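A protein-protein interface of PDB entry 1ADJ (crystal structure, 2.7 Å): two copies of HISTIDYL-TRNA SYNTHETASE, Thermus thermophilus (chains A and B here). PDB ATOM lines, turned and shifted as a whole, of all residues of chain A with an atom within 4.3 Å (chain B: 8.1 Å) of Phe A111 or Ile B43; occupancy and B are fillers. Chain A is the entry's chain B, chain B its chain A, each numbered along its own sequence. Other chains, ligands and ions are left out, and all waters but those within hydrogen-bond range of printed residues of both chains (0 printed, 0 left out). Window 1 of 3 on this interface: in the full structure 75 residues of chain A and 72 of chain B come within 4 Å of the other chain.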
ATOM      1  N   ILE A  43       7.158 -29.950 -20.801  1.00  0.00           N
ATOM      2  CA  ILE A  43       6.923 -28.580 -21.236  1.00  0.00           C
ATOM      3  C   ILE A  43       6.577 -28.523 -22.728  1.00  0.00           C
ATOM      4  O   ILE A  43       5.933 -27.578 -23.195  1.00  0.00           O
ATOM      5  CB  ILE A  43       8.157 -27.694 -20.898  1.00  0.00           C
ATOM      6  CG1 ILE A  43       8.269 -27.517 -19.379  1.00  0.00           C
ATOM      7  CG2 ILE A  43       8.076 -26.330 -21.587  1.00  0.00           C
ATOM      8  CD1 ILE A  43       7.218 -26.613 -18.774  1.00  0.00           C
ATOM      9  N   PHE A  66       4.367 -21.654 -29.707  1.00  0.00           N
ATOM     10  CA  PHE A  66       5.815 -21.542 -29.820  1.00  0.00           C
ATOM     11  C   PHE A  66       6.287 -22.912 -30.270  1.00  0.00           C
ATOM     12  O   PHE A  66       6.443 -23.822 -29.457  1.00  0.00           O
ATOM     13  CB  PHE A  66       6.452 -21.203 -28.475  1.00  0.00           C
ATOM     14  CG  PHE A  66       6.267 -19.776 -28.057  1.00  0.00           C
ATOM     15  CD1 PHE A  66       6.775 -18.743 -28.829  1.00  0.00           C
ATOM     16  CD2 PHE A  66       5.597 -19.467 -26.878  1.00  0.00           C
ATOM     17  CE1 PHE A  66       6.622 -17.420 -28.434  1.00  0.00           C
ATOM     18  CE2 PHE A  66       5.438 -18.150 -26.473  1.00  0.00           C
ATOM     19  CZ  PHE A  66       5.953 -17.121 -27.254  1.00  0.00           C
ATOM     20  N   LEU A  78       5.862 -25.843 -27.584  1.00  0.00           N
ATOM     21  CA  LEU A  78       5.701 -25.444 -26.196  1.00  0.00           C
ATOM     22  C   LEU A  78       4.213 -25.516 -25.868  1.00  0.00           C
ATOM     23  O   LEU A  78       3.391 -24.831 -26.494  1.00  0.00           O
ATOM     24  CB  LEU A  78       6.209 -24.011 -26.014  1.00  0.00           C
ATOM     25  CG  LEU A  78       7.590 -23.801 -25.390  1.00  0.00           C
ATOM     26  CD1 LEU A  78       8.602 -24.760 -25.971  1.00  0.00           C
ATOM     27  CD2 LEU A  78       8.019 -22.351 -25.582  1.00  0.00           C
ATOM     28  N   ARG A  79       3.877 -26.379 -24.917  1.00  0.00           N
ATOM     29  CA  ARG A  79       2.503 -26.598 -24.482  1.00  0.00           C
ATOM     30  C   ARG A  79       1.707 -25.311 -24.255  1.00  0.00           C
ATOM     31  O   ARG A  79       2.065 -24.479 -23.422  1.00  0.00           O
ATOM     32  CB  ARG A  79       2.517 -27.483 -23.233  1.00  0.00           C
ATOM     33  CG  ARG A  79       1.410 -27.244 -22.253  1.00  0.00           C
ATOM     34  CD  ARG A  79       1.984 -26.916 -20.876  1.00  0.00           C
ATOM     35  NE  ARG A  79       2.462 -28.104 -20.171  1.00  0.00           N
ATOM     36  CZ  ARG A  79       2.930 -28.102 -18.925  1.00  0.00           C
ATOM     37  NH1 ARG A  79       2.991 -26.975 -18.232  1.00  0.00           N
ATOM     38  NH2 ARG A  79       3.313 -29.237 -18.363  1.00  0.00           N
ATOM     39  N   PRO A  80       0.645 -25.106 -25.054  1.00  0.00           N
ATOM     40  CA  PRO A  80      -0.220 -23.923 -24.963  1.00  0.00           C
ATOM     41  C   PRO A  80      -1.450 -24.165 -24.091  1.00  0.00           C
ATOM     42  O   PRO A  80      -2.139 -23.221 -23.708  1.00  0.00           O
ATOM     43  CB  PRO A  80      -0.633 -23.712 -26.410  1.00  0.00           C
ATOM     44  CG  PRO A  80      -0.827 -25.117 -26.872  1.00  0.00           C
ATOM     45  CD  PRO A  80       0.358 -25.863 -26.287  1.00  0.00           C
ATOM     46  N   PRO A 109       3.223 -23.948 -16.103  1.00  0.00           N
ATOM     47  CA  PRO A 109       3.265 -22.889 -17.109  1.00  0.00           C
ATOM     48  C   PRO A 109       2.707 -23.331 -18.464  1.00  0.00           C
ATOM     49  O   PRO A 109       2.835 -24.491 -18.854  1.00  0.00           O
ATOM     50  CB  PRO A 109       4.752 -22.552 -17.168  1.00  0.00           C
ATOM     51  CG  PRO A 109       5.392 -23.880 -16.906  1.00  0.00           C
ATOM     52  CD  PRO A 109       4.582 -24.417 -15.772  1.00  0.00           C
ATOM     53  N   MET A 110       2.053 -22.404 -19.156  1.00  0.00           N
ATOM     54  CA  MET A 110       1.469 -22.658 -20.470  1.00  0.00           C
ATOM     55  C   MET A 110       2.023 -21.530 -21.315  1.00  0.00           C
ATOM     56  O   MET A 110       2.199 -20.410 -20.811  1.00  0.00           O
ATOM     57  CB  MET A 110      -0.060 -22.571 -20.416  1.00  0.00           C
ATOM     58  CG  MET A 110      -0.738 -23.651 -19.591  1.00  0.00           C
ATOM     59  SD  MET A 110      -0.486 -25.307 -20.282  1.00  0.00           S
ATOM     60  CE  MET A 110      -1.003 -26.367 -18.913  1.00  0.00           C
ATOM     61  N   PHE A 111       2.273 -21.799 -22.596  1.00  0.00           N
ATOM     62  CA  PHE A 111       2.863 -20.787 -23.472  1.00  0.00           C
ATOM     63  C   PHE A 111       2.040 -20.512 -24.714  1.00  0.00           C
ATOM     64  O   PHE A 111       1.611 -21.433 -25.412  1.00  0.00           O
ATOM     65  CB  PHE A 111       4.284 -21.211 -23.874  1.00  0.00           C
ATOM     66  CG  PHE A 111       5.053 -21.848 -22.755  1.00  0.00           C
ATOM     67  CD1 PHE A 111       4.950 -23.216 -22.518  1.00  0.00           C
ATOM     68  CD2 PHE A 111       5.798 -21.072 -21.878  1.00  0.00           C
ATOM     69  CE1 PHE A 111       5.570 -23.802 -21.420  1.00  0.00           C
ATOM     70  CE2 PHE A 111       6.426 -21.651 -20.769  1.00  0.00           C
ATOM     71  CZ  PHE A 111       6.308 -23.017 -20.540  1.00  0.00           C
ATOM     72  N   ARG A 112       1.862 -19.229 -24.997  1.00  0.00           N
ATOM     73  CA  ARG A 112       1.118 -18.789 -26.156  1.00  0.00           C
ATOM     74  C   ARG A 112       1.793 -17.611 -26.854  1.00  0.00           C
ATOM     75  O   ARG A 112       1.976 -16.545 -26.268  1.00  0.00           O
ATOM     76  CB  ARG A 112      -0.319 -18.439 -25.765  1.00  0.00           C
ATOM     77  CG  ARG A 112      -1.317 -19.398 -26.377  1.00  0.00           C
ATOM     78  CD  ARG A 112      -1.858 -20.367 -25.372  1.00  0.00           C
ATOM     79  NE  ARG A 112      -3.039 -19.802 -24.741  1.00  0.00           N
ATOM     80  CZ  ARG A 112      -4.153 -20.482 -24.496  1.00  0.00           C
ATOM     81  NH1 ARG A 112      -4.240 -21.761 -24.823  1.00  0.00           N
ATOM     82  NH2 ARG A 112      -5.191 -19.878 -23.934  1.00  0.00           N
ATOM     83  N   ARG A 122       2.617 -14.324 -22.419  1.00  0.00           N
ATOM     84  CA  ARG A 122       3.094 -15.302 -23.388  1.00  0.00           C
ATOM     85  C   ARG A 122       3.431 -16.572 -22.608  1.00  0.00           C
ATOM     86  O   ARG A 122       3.504 -17.667 -23.164  1.00  0.00           O
ATOM     87  CB  ARG A 122       4.285 -14.770 -24.176  1.00  0.00           C
ATOM     88  CG  ARG A 122       3.865 -14.128 -25.487  1.00  0.00           C
ATOM     89  CD  ARG A 122       4.499 -12.764 -25.708  1.00  0.00           C
ATOM     90  NE  ARG A 122       5.948 -12.839 -25.880  1.00  0.00           N
ATOM     91  CZ  ARG A 122       6.556 -13.396 -26.920  1.00  0.00           C
ATOM     92  NH1 ARG A 122       5.851 -13.941 -27.900  1.00  0.00           N
ATOM     93  NH2 ARG A 122       7.878 -13.403 -26.982  1.00  0.00           N
ATOM     94  N   GLN A 123       3.661 -16.401 -21.308  1.00  0.00           N
ATOM     95  CA  GLN A 123       3.908 -17.519 -20.401  1.00  0.00           C
ATOM     96  C   GLN A 123       3.049 -17.244 -19.185  1.00  0.00           C
ATOM     97  O   GLN A 123       3.292 -16.277 -18.462  1.00  0.00           O
ATOM     98  CB  GLN A 123       5.366 -17.635 -19.937  1.00  0.00           C
ATOM     99  CG  GLN A 123       5.536 -18.848 -19.002  1.00  0.00           C
ATOM    100  CD  GLN A 123       6.888 -18.949 -18.327  1.00  0.00           C
ATOM    101  OE1 GLN A 123       7.914 -19.102 -18.978  1.00  0.00           O
ATOM    102  NE2 GLN A 123       6.888 -18.893 -17.009  1.00  0.00           N
ATOM    103  N   VAL B  40      11.632 -17.415  -9.296  1.00  0.00           N
ATOM    104  CA  VAL B  40      11.426 -18.284 -10.449  1.00  0.00           C
ATOM    105  C   VAL B  40      11.473 -17.465 -11.732  1.00  0.00           C
ATOM    106  O   VAL B  40      10.692 -16.537 -11.905  1.00  0.00           O
ATOM    107  CB  VAL B  40      10.078 -19.028 -10.360  1.00  0.00           C
ATOM    108  CG1 VAL B  40       9.970 -20.038 -11.477  1.00  0.00           C
ATOM    109  CG2 VAL B  40       9.951 -19.724  -9.013  1.00  0.00           C
ATOM    110  N   THR B  41      12.430 -17.774 -12.597  1.00  0.00           N
ATOM    111  CA  THR B  41      12.581 -17.065 -13.859  1.00  0.00           C
ATOM    112  C   THR B  41      11.778 -17.777 -14.948  1.00  0.00           C
ATOM    113  O   THR B  41      11.457 -18.961 -14.806  1.00  0.00           O
ATOM    114  CB  THR B  41      14.066 -16.988 -14.285  1.00  0.00           C
ATOM    115  OG1 THR B  41      14.623 -18.308 -14.356  1.00  0.00           O
ATOM    116  CG2 THR B  41      14.855 -16.173 -13.295  1.00  0.00           C
ATOM    117  N   PRO B  42      11.439 -17.068 -16.045  1.00  0.00           N
ATOM    118  CA  PRO B  42      10.673 -17.634 -17.160  1.00  0.00           C
ATOM    119  C   PRO B  42      11.336 -18.871 -17.757  1.00  0.00           C
ATOM    120  O   PRO B  42      12.529 -19.085 -17.580  1.00  0.00           O
ATOM    121  CB  PRO B  42      10.652 -16.490 -18.161  1.00  0.00           C
ATOM    122  CG  PRO B  42      10.635 -15.289 -17.286  1.00  0.00           C
ATOM    123  CD  PRO B  42      11.686 -15.632 -16.275  1.00  0.00           C
ATOM    124  N   ILE B  43      10.559 -19.672 -18.473  1.00  0.00           N
ATOM    125  CA  ILE B  43      11.054 -20.895 -19.096  1.00  0.00           C
ATOM    126  C   ILE B  43      12.030 -20.588 -20.235  1.00  0.00           C
ATOM    127  O   ILE B  43      12.863 -21.423 -20.591  1.00  0.00           O
ATOM    128  CB  ILE B  43       9.869 -21.762 -19.590  1.00  0.00           C
ATOM    129  CG1 ILE B  43       9.100 -22.317 -18.387  1.00  0.00           C
ATOM    130  CG2 ILE B  43      10.341 -22.900 -20.484  1.00  0.00           C
ATOM    131  CD1 ILE B  43       9.825 -23.402 -17.632  1.00  0.00           C
ATOM    132  N   PHE B  44      11.926 -19.396 -20.813  1.00  0.00           N
ATOM    133  CA  PHE B  44      12.827 -19.000 -21.891  1.00  0.00           C
ATOM    134  C   PHE B  44      13.309 -17.566 -21.721  1.00  0.00           C
ATOM    135  O   PHE B  44      12.654 -16.744 -21.066  1.00  0.00           O
ATOM    136  CB  PHE B  44      12.219 -19.237 -23.298  1.00  0.00           C
ATOM    137  CG  PHE B  44      10.818 -18.710 -23.475  1.00  0.00           C
ATOM    138  CD1 PHE B  44      10.560 -17.342 -23.481  1.00  0.00           C
ATOM    139  CD2 PHE B  44       9.755 -19.591 -23.639  1.00  0.00           C
ATOM    140  CE1 PHE B  44       9.262 -16.855 -23.648  1.00  0.00           C
ATOM    141  CE2 PHE B  44       8.445 -19.116 -23.808  1.00  0.00           C
ATOM    142  CZ  PHE B  44       8.201 -17.744 -23.812  1.00  0.00           C
ATOM    143  N   GLU B  45      14.487 -17.296 -22.270  1.00  0.00           N
ATOM    144  CA  GLU B  45      15.105 -15.977 -22.208  1.00  0.00           C
ATOM    145  C   GLU B  45      15.537 -15.610 -23.625  1.00  0.00           C
ATOM    146  O   GLU B  45      15.479 -16.455 -24.531  1.00  0.00           O
ATOM    147  CB  GLU B  45      16.364 -16.027 -21.329  1.00  0.00           C
ATOM    148  CG  GLU B  45      16.149 -16.383 -19.863  1.00  0.00           C
ATOM    149  CD  GLU B  45      15.844 -15.173 -18.985  1.00  0.00           C
ATOM    150  OE1 GLU B  45      16.011 -14.021 -19.451  1.00  0.00           O
ATOM    151  OE2 GLU B  45      15.447 -15.378 -17.814  1.00  0.00           O
ATOM    152  N   PHE B  50      21.955 -16.662 -22.777  1.00  0.00           N
ATOM    153  CA  PHE B  50      22.687 -17.911 -22.651  1.00  0.00           C
ATOM    154  C   PHE B  50      23.941 -17.948 -23.521  1.00  0.00           C
ATOM    155  O   PHE B  50      24.926 -18.585 -23.154  1.00  0.00           O
ATOM    156  CB  PHE B  50      21.777 -19.103 -22.951  1.00  0.00           C
ATOM    157  CG  PHE B  50      20.561 -19.160 -22.075  1.00  0.00           C
ATOM    158  CD1 PHE B  50      20.689 -19.150 -20.687  1.00  0.00           C
ATOM    159  CD2 PHE B  50      19.284 -19.180 -22.632  1.00  0.00           C
ATOM    160  CE1 PHE B  50      19.563 -19.153 -19.863  1.00  0.00           C
ATOM    161  CE2 PHE B  50      18.147 -19.186 -21.815  1.00  0.00           C
ATOM    162  CZ  PHE B  50      18.289 -19.171 -20.429  1.00  0.00           C
ATOM    163  N   PHE B  66      17.569 -25.527 -27.000  1.00  0.00           N
ATOM    164  CA  PHE B  66      16.336 -25.508 -27.778  1.00  0.00           C
ATOM    165  C   PHE B  66      16.041 -24.042 -28.028  1.00  0.00           C
ATOM    166  O   PHE B  66      15.489 -23.355 -27.172  1.00  0.00           O
ATOM    167  CB  PHE B  66      15.183 -26.137 -27.001  1.00  0.00           C
ATOM    168  CG  PHE B  66      15.247 -27.626 -26.920  1.00  0.00           C
ATOM    169  CD1 PHE B  66      15.195 -28.390 -28.075  1.00  0.00           C
ATOM    170  CD2 PHE B  66      15.338 -28.268 -25.693  1.00  0.00           C
ATOM    171  CE1 PHE B  66      15.230 -29.780 -28.011  1.00  0.00           C
ATOM    172  CE2 PHE B  66      15.374 -29.655 -25.617  1.00  0.00           C
ATOM    173  CZ  PHE B  66      15.319 -30.414 -26.781  1.00  0.00           C
ATOM    174  N   PHE B  68      14.442 -21.042 -30.683  1.00  0.00           N
ATOM    175  CA  PHE B  68      13.452 -20.836 -31.734  1.00  0.00           C
ATOM    176  C   PHE B  68      13.204 -19.341 -31.894  1.00  0.00           C
ATOM    177  O   PHE B  68      13.693 -18.535 -31.108  1.00  0.00           O
ATOM    178  CB  PHE B  68      12.139 -21.547 -31.365  1.00  0.00           C
ATOM    179  CG  PHE B  68      11.592 -21.156 -30.018  1.00  0.00           C
ATOM    180  CD1 PHE B  68      10.763 -20.049 -29.884  1.00  0.00           C
ATOM    181  CD2 PHE B  68      11.942 -21.871 -28.877  1.00  0.00           C
ATOM    182  CE1 PHE B  68      10.295 -19.656 -28.641  1.00  0.00           C
ATOM    183  CE2 PHE B  68      11.479 -21.487 -27.632  1.00  0.00           C
ATOM    184  CZ  PHE B  68      10.654 -20.377 -27.511  1.00  0.00           C
ATOM    185  N   LEU B  76      14.495 -16.616 -29.062  1.00  0.00           N
ATOM    186  CA  LEU B  76      14.243 -17.057 -27.693  1.00  0.00           C
ATOM    187  C   LEU B  76      14.813 -18.455 -27.500  1.00  0.00           C
ATOM    188  O   LEU B  76      14.813 -19.264 -28.434  1.00  0.00           O
ATOM    189  CB  LEU B  76      12.735 -17.074 -27.413  1.00  0.00           C
ATOM    190  CG  LEU B  76      12.005 -15.811 -26.928  1.00  0.00           C
ATOM    191  CD1 LEU B  76      12.770 -14.534 -27.247  1.00  0.00           C
ATOM    192  CD2 LEU B  76      10.618 -15.785 -27.537  1.00  0.00           C
ATOM    193  N   THR B  77      15.276 -18.754 -26.291  1.00  0.00           N
ATOM    194  CA  THR B  77      15.849 -20.062 -26.013  1.00  0.00           C
ATOM    195  C   THR B  77      15.365 -20.655 -24.703  1.00  0.00           C
ATOM    196  O   THR B  77      15.245 -19.960 -23.689  1.00  0.00           O
ATOM    197  CB  THR B  77      17.387 -20.000 -26.007  1.00  0.00           C
ATOM    198  OG1 THR B  77      17.848 -19.589 -27.300  1.00  0.00           O
ATOM    199  CG2 THR B  77      17.983 -21.354 -25.690  1.00  0.00           C
ATOM    200  N   LEU B  78      15.026 -21.939 -24.760  1.00  0.00           N
ATOM    201  CA  LEU B  78      14.577 -22.693 -23.600  1.00  0.00           C
ATOM    202  C   LEU B  78      15.765 -22.801 -22.651  1.00  0.00           C
ATOM    203  O   LEU B  78      16.823 -23.341 -23.008  1.00  0.00           O
ATOM    204  CB  LEU B  78      14.119 -24.094 -24.023  1.00  0.00           C
ATOM    205  CG  LEU B  78      12.623 -24.366 -24.193  1.00  0.00           C
ATOM    206  CD1 LEU B  78      11.940 -23.224 -24.911  1.00  0.00           C
ATOM    207  CD2 LEU B  78      12.417 -25.683 -24.928  1.00  0.00           C
ATOM    208  N   ARG B  79      15.589 -22.236 -21.464  1.00  0.00           N
ATOM    209  CA  ARG B  79      16.596 -22.225 -20.404  1.00  0.00           C
ATOM    210  C   ARG B  79      17.272 -23.583 -20.187  1.00  0.00           C
ATOM    211  O   ARG B  79      16.622 -24.579 -19.846  1.00  0.00           O
ATOM    212  CB  ARG B  79      15.955 -21.696 -19.105  1.00  0.00           C
ATOM    213  CG  ARG B  79      16.507 -22.273 -17.828  1.00  0.00           C
ATOM    214  CD  ARG B  79      15.402 -22.919 -17.005  1.00  0.00           C
ATOM    215  NE  ARG B  79      14.592 -21.934 -16.300  1.00  0.00           N
ATOM    216  CZ  ARG B  79      13.600 -22.231 -15.468  1.00  0.00           C
ATOM    217  NH1 ARG B  79      13.286 -23.489 -15.226  1.00  0.00           N
ATOM    218  NH2 ARG B  79      12.921 -21.260 -14.876  1.00  0.00           N
ATOM    219  N   PRO B  80      18.585 -23.648 -20.449  1.00  0.00           N
ATOM    220  CA  PRO B  80      19.386 -24.869 -20.291  1.00  0.00           C
ATOM    221  C   PRO B  80      20.073 -24.945 -18.929  1.00  0.00           C
ATOM    222  O   PRO B  80      20.563 -26.000 -18.530  1.00  0.00           O
ATOM    223  CB  PRO B  80      20.417 -24.725 -21.400  1.00  0.00           C
ATOM    224  CG  PRO B  80      20.708 -23.264 -21.355  1.00  0.00           C
ATOM    225  CD  PRO B  80      19.341 -22.619 -21.183  1.00  0.00           C
ATOM    226  N   GLU B  81      20.074 -23.823 -18.213  1.00  0.00           N
ATOM    227  CA  GLU B  81      20.719 -23.702 -16.913  1.00  0.00           C
ATOM    228  C   GLU B  81      20.176 -22.441 -16.235  1.00  0.00           C
ATOM    229  O   GLU B  81      19.704 -21.527 -16.917  1.00  0.00           O
ATOM    230  CB  GLU B  81      22.236 -23.658 -17.134  1.00  0.00           C
ATOM    231  CG  GLU B  81      23.059 -22.816 -16.179  1.00  0.00           C
ATOM    232  CD  GLU B  81      23.203 -21.378 -16.629  1.00  0.00           C
ATOM    233  OE1 GLU B  81      22.975 -21.072 -17.820  1.00  0.00           O
ATOM    234  OE2 GLU B  81      23.554 -20.544 -15.783  1.00  0.00           O
ATOM    235  N   ALA B  85      20.215 -16.680 -15.974  1.00  0.00           N
ATOM    236  CA  ALA B  85      18.872 -16.135 -15.795  1.00  0.00           C
ATOM    237  C   ALA B  85      18.760 -15.412 -14.458  1.00  0.00           C
ATOM    238  O   ALA B  85      18.199 -14.313 -14.373  1.00  0.00           O
ATOM    239  CB  ALA B  85      17.838 -17.240 -15.886  1.00  0.00           C
ATOM    240  N   ARG B  88      20.479 -12.250 -14.685  1.00  0.00           N
ATOM    241  CA  ARG B  88      19.671 -11.390 -15.557  1.00  0.00           C
ATOM    242  C   ARG B  88      18.571 -10.768 -14.706  1.00  0.00           C
ATOM    243  O   ARG B  88      18.305  -9.567 -14.794  1.00  0.00           O
ATOM    244  CB  ARG B  88      19.073 -12.224 -16.697  1.00  0.00           C
ATOM    245  CG  ARG B  88      18.421 -11.430 -17.842  1.00  0.00           C
ATOM    246  CD  ARG B  88      16.952 -11.086 -17.569  1.00  0.00           C
ATOM    247  NE  ARG B  88      16.163 -12.270 -17.240  1.00  0.00           N
ATOM    248  CZ  ARG B  88      15.207 -12.293 -16.318  1.00  0.00           C
ATOM    249  NH1 ARG B  88      14.908 -11.199 -15.634  1.00  0.00           N
ATOM    250  NH2 ARG B  88      14.589 -13.425 -16.041  1.00  0.00           N
ATOM    251  N   GLY B 108      13.217 -25.952 -10.816  1.00  0.00           N
ATOM    252  CA  GLY B 108      12.409 -25.989 -12.020  1.00  0.00           C
ATOM    253  C   GLY B 108      13.029 -26.792 -13.134  1.00  0.00           C
ATOM    254  O   GLY B 108      14.117 -27.348 -12.974  1.00  0.00           O
ATOM    255  N   PRO B 109      12.323 -26.931 -14.263  1.00  0.00           N
ATOM    256  CA  PRO B 109      12.812 -27.685 -15.420  1.00  0.00           C
ATOM    257  C   PRO B 109      13.891 -26.950 -16.210  1.00  0.00           C
ATOM    258  O   PRO B 109      13.867 -25.727 -16.328  1.00  0.00           O
ATOM    259  CB  PRO B 109      11.542 -27.883 -16.245  1.00  0.00           C
ATOM    260  CG  PRO B 109      10.761 -26.633 -15.954  1.00  0.00           C
ATOM    261  CD  PRO B 109      10.933 -26.483 -14.468  1.00  0.00           C
ATOM    262  N   MET B 110      14.841 -27.708 -16.738  1.00  0.00           N
ATOM    263  CA  MET B 110      15.933 -27.162 -17.535  1.00  0.00           C
ATOM    264  C   MET B 110      15.892 -27.984 -18.810  1.00  0.00           C
ATOM    265  O   MET B 110      15.555 -29.178 -18.767  1.00  0.00           O
ATOM    266  CB  MET B 110      17.267 -27.352 -16.814  1.00  0.00           C
ATOM    267  CG  MET B 110      17.409 -26.555 -15.532  1.00  0.00           C
ATOM    268  SD  MET B 110      17.384 -24.772 -15.826  1.00  0.00           S
ATOM    269  CE  MET B 110      17.172 -24.153 -14.152  1.00  0.00           C
ATOM    270  N   PHE B 111      16.229 -27.368 -19.938  1.00  0.00           N
ATOM    271  CA  PHE B 111      16.161 -28.071 -21.216  1.00  0.00           C
ATOM    272  C   PHE B 111      17.465 -28.076 -21.992  1.00  0.00           C
ATOM    273  O   PHE B 111      18.093 -27.033 -22.190  1.00  0.00           O
ATOM    274  CB  PHE B 111      15.050 -27.465 -22.086  1.00  0.00           C
ATOM    275  CG  PHE B 111      13.827 -27.097 -21.313  1.00  0.00           C
ATOM    276  CD1 PHE B 111      12.832 -28.042 -21.070  1.00  0.00           C
ATOM    277  CD2 PHE B 111      13.711 -25.832 -20.740  1.00  0.00           C
ATOM    278  CE1 PHE B 111      11.747 -27.734 -20.260  1.00  0.00           C
ATOM    279  CE2 PHE B 111      12.625 -25.510 -19.926  1.00  0.00           C
ATOM    280  CZ  PHE B 111      11.642 -26.463 -19.682  1.00  0.00           C
ATOM    281  N   GLN B 123      14.739 -32.810 -20.875  1.00  0.00           N
ATOM    282  CA  GLN B 123      14.045 -31.953 -19.924  1.00  0.00           C
ATOM    283  C   GLN B 123      14.279 -32.591 -18.564  1.00  0.00           C
ATOM    284  O   GLN B 123      13.784 -33.693 -18.293  1.00  0.00           O
ATOM    285  CB  GLN B 123      12.534 -31.857 -20.158  1.00  0.00           C
ATOM    286  CG  GLN B 123      11.894 -30.925 -19.128  1.00  0.00           C
ATOM    287  CD  GLN B 123      10.383 -30.934 -19.122  1.00  0.00           C
ATOM    288  OE1 GLN B 123       9.741 -30.558 -20.097  1.00  0.00           O
ATOM    289  NE2 GLN B 123       9.805 -31.337 -18.004  1.00  0.00           N
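Ile A43 touches Phe B111, and with the chains exchanged Phe A111 touches Ile B43.
Ile A43 touches Gln B123, and with the chains exchanged Gln A123 touches Ile B43.
Leu B78 touches its own counterpart, Leu A78.
Positions printed for both chains: 43, 66, 78, 79, 80, 109, 110, 111 and 123.
CZ of Phe B111 touches CG1 of Ile A43, at 3.5 Å.
Phe B44 touches Phe A66.
Phe A66 touches Phe B68 (CD1 to CE1, 3.6 Å).
CD2 of Leu A78 touches CE2 of Phe B44 (3.7 Å).
Phe B68 touches Leu A78.
Leu A78 touches Leu B78 (CD1 to CD1, 3.8 Å).
Phe A111 touches Ile B43 (CZ to CG1, 3.6 Å).
Phe A111 touches Phe B44.
CD2 of Leu B76 touches NH2 of Arg A122, 3.7 Å away.
Gln A123 touches Pro B42 (OE1 to CA, 3.6 Å).
OE1 of Gln A123 sits at hydrogen-bond distance from N of Ile B43 (2.8 Å).
The backbone NH (N) of Ile A43 is in hydrogen-bond range of the side-chain amide oxygen (OE1) of Gln B123 (2.7 Å).
Of the printed residues of chain B, Ile A43 touches Phe B111 (3.5 Å) and Gln B123 (2.7 Å).
Of the printed residues of chain B, Phe A66 touches Phe B44 and Phe B68.
Phe A111 touches just these residues of chain B: Ile B43 and Phe B44.
Of the printed residues of chain B, Arg A122 touches Leu B76.
Ile B43 touches just these residues of chain A: Phe A111 and Gln A123.
Glu B45 touches none of the printed residues of chain A.
Arg B79 touches none of the printed residues of chain A.
Of the printed residues of chain A, Phe B111 touches Ile A43 (3.5 Å).
Of the printed residues of chain A, Gln B123 touches Ile A43 (2.7 Å).
The nearest printed residue of chain A that does not touch Ile B43 is Ile A43 (4.3 Å).
Of the 22 printed residues of chain B, 8 touch a printed residue of chain A.
Hydrophobic or aromatic side chains of chain B that line the printed part of chain A: Pro B42, Ile B43, Phe B44, Phe B68, Leu B76, Leu B78 and Phe B111.
Among the printed residues, 12 pairs touch across the chains.
Among the printed residues, no Asp or Glu carboxylate lies within 4 Å of a Lys or Arg side-chain nitrogen of the other chain.
O of Ile B43 sits at hydrogen-bond distance from N of Arg B79, at 3.0 Å.
The backbone carbonyl oxygen of Leu B76 sits at hydrogen-bond distance from the backbone NH of Phe B68 (2.9 Å).
The backbone carbonyl oxygen of Arg B79 sits at hydrogen-bond distance from the backbone NH of Phe B111.
The backbone carbonyl oxygen (O) of Ile A43 is in hydrogen-bond range of the backbone NH (N) of Arg A79, at 2.9 Å.
The backbone carbonyl oxygen (O) of Phe A66 is in hydrogen-bond range of the backbone NH (N) of Leu A78 (2.8 Å).
The backbone NH of Arg A112 is in hydrogen-bond range of the backbone carbonyl oxygen of Arg A122.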
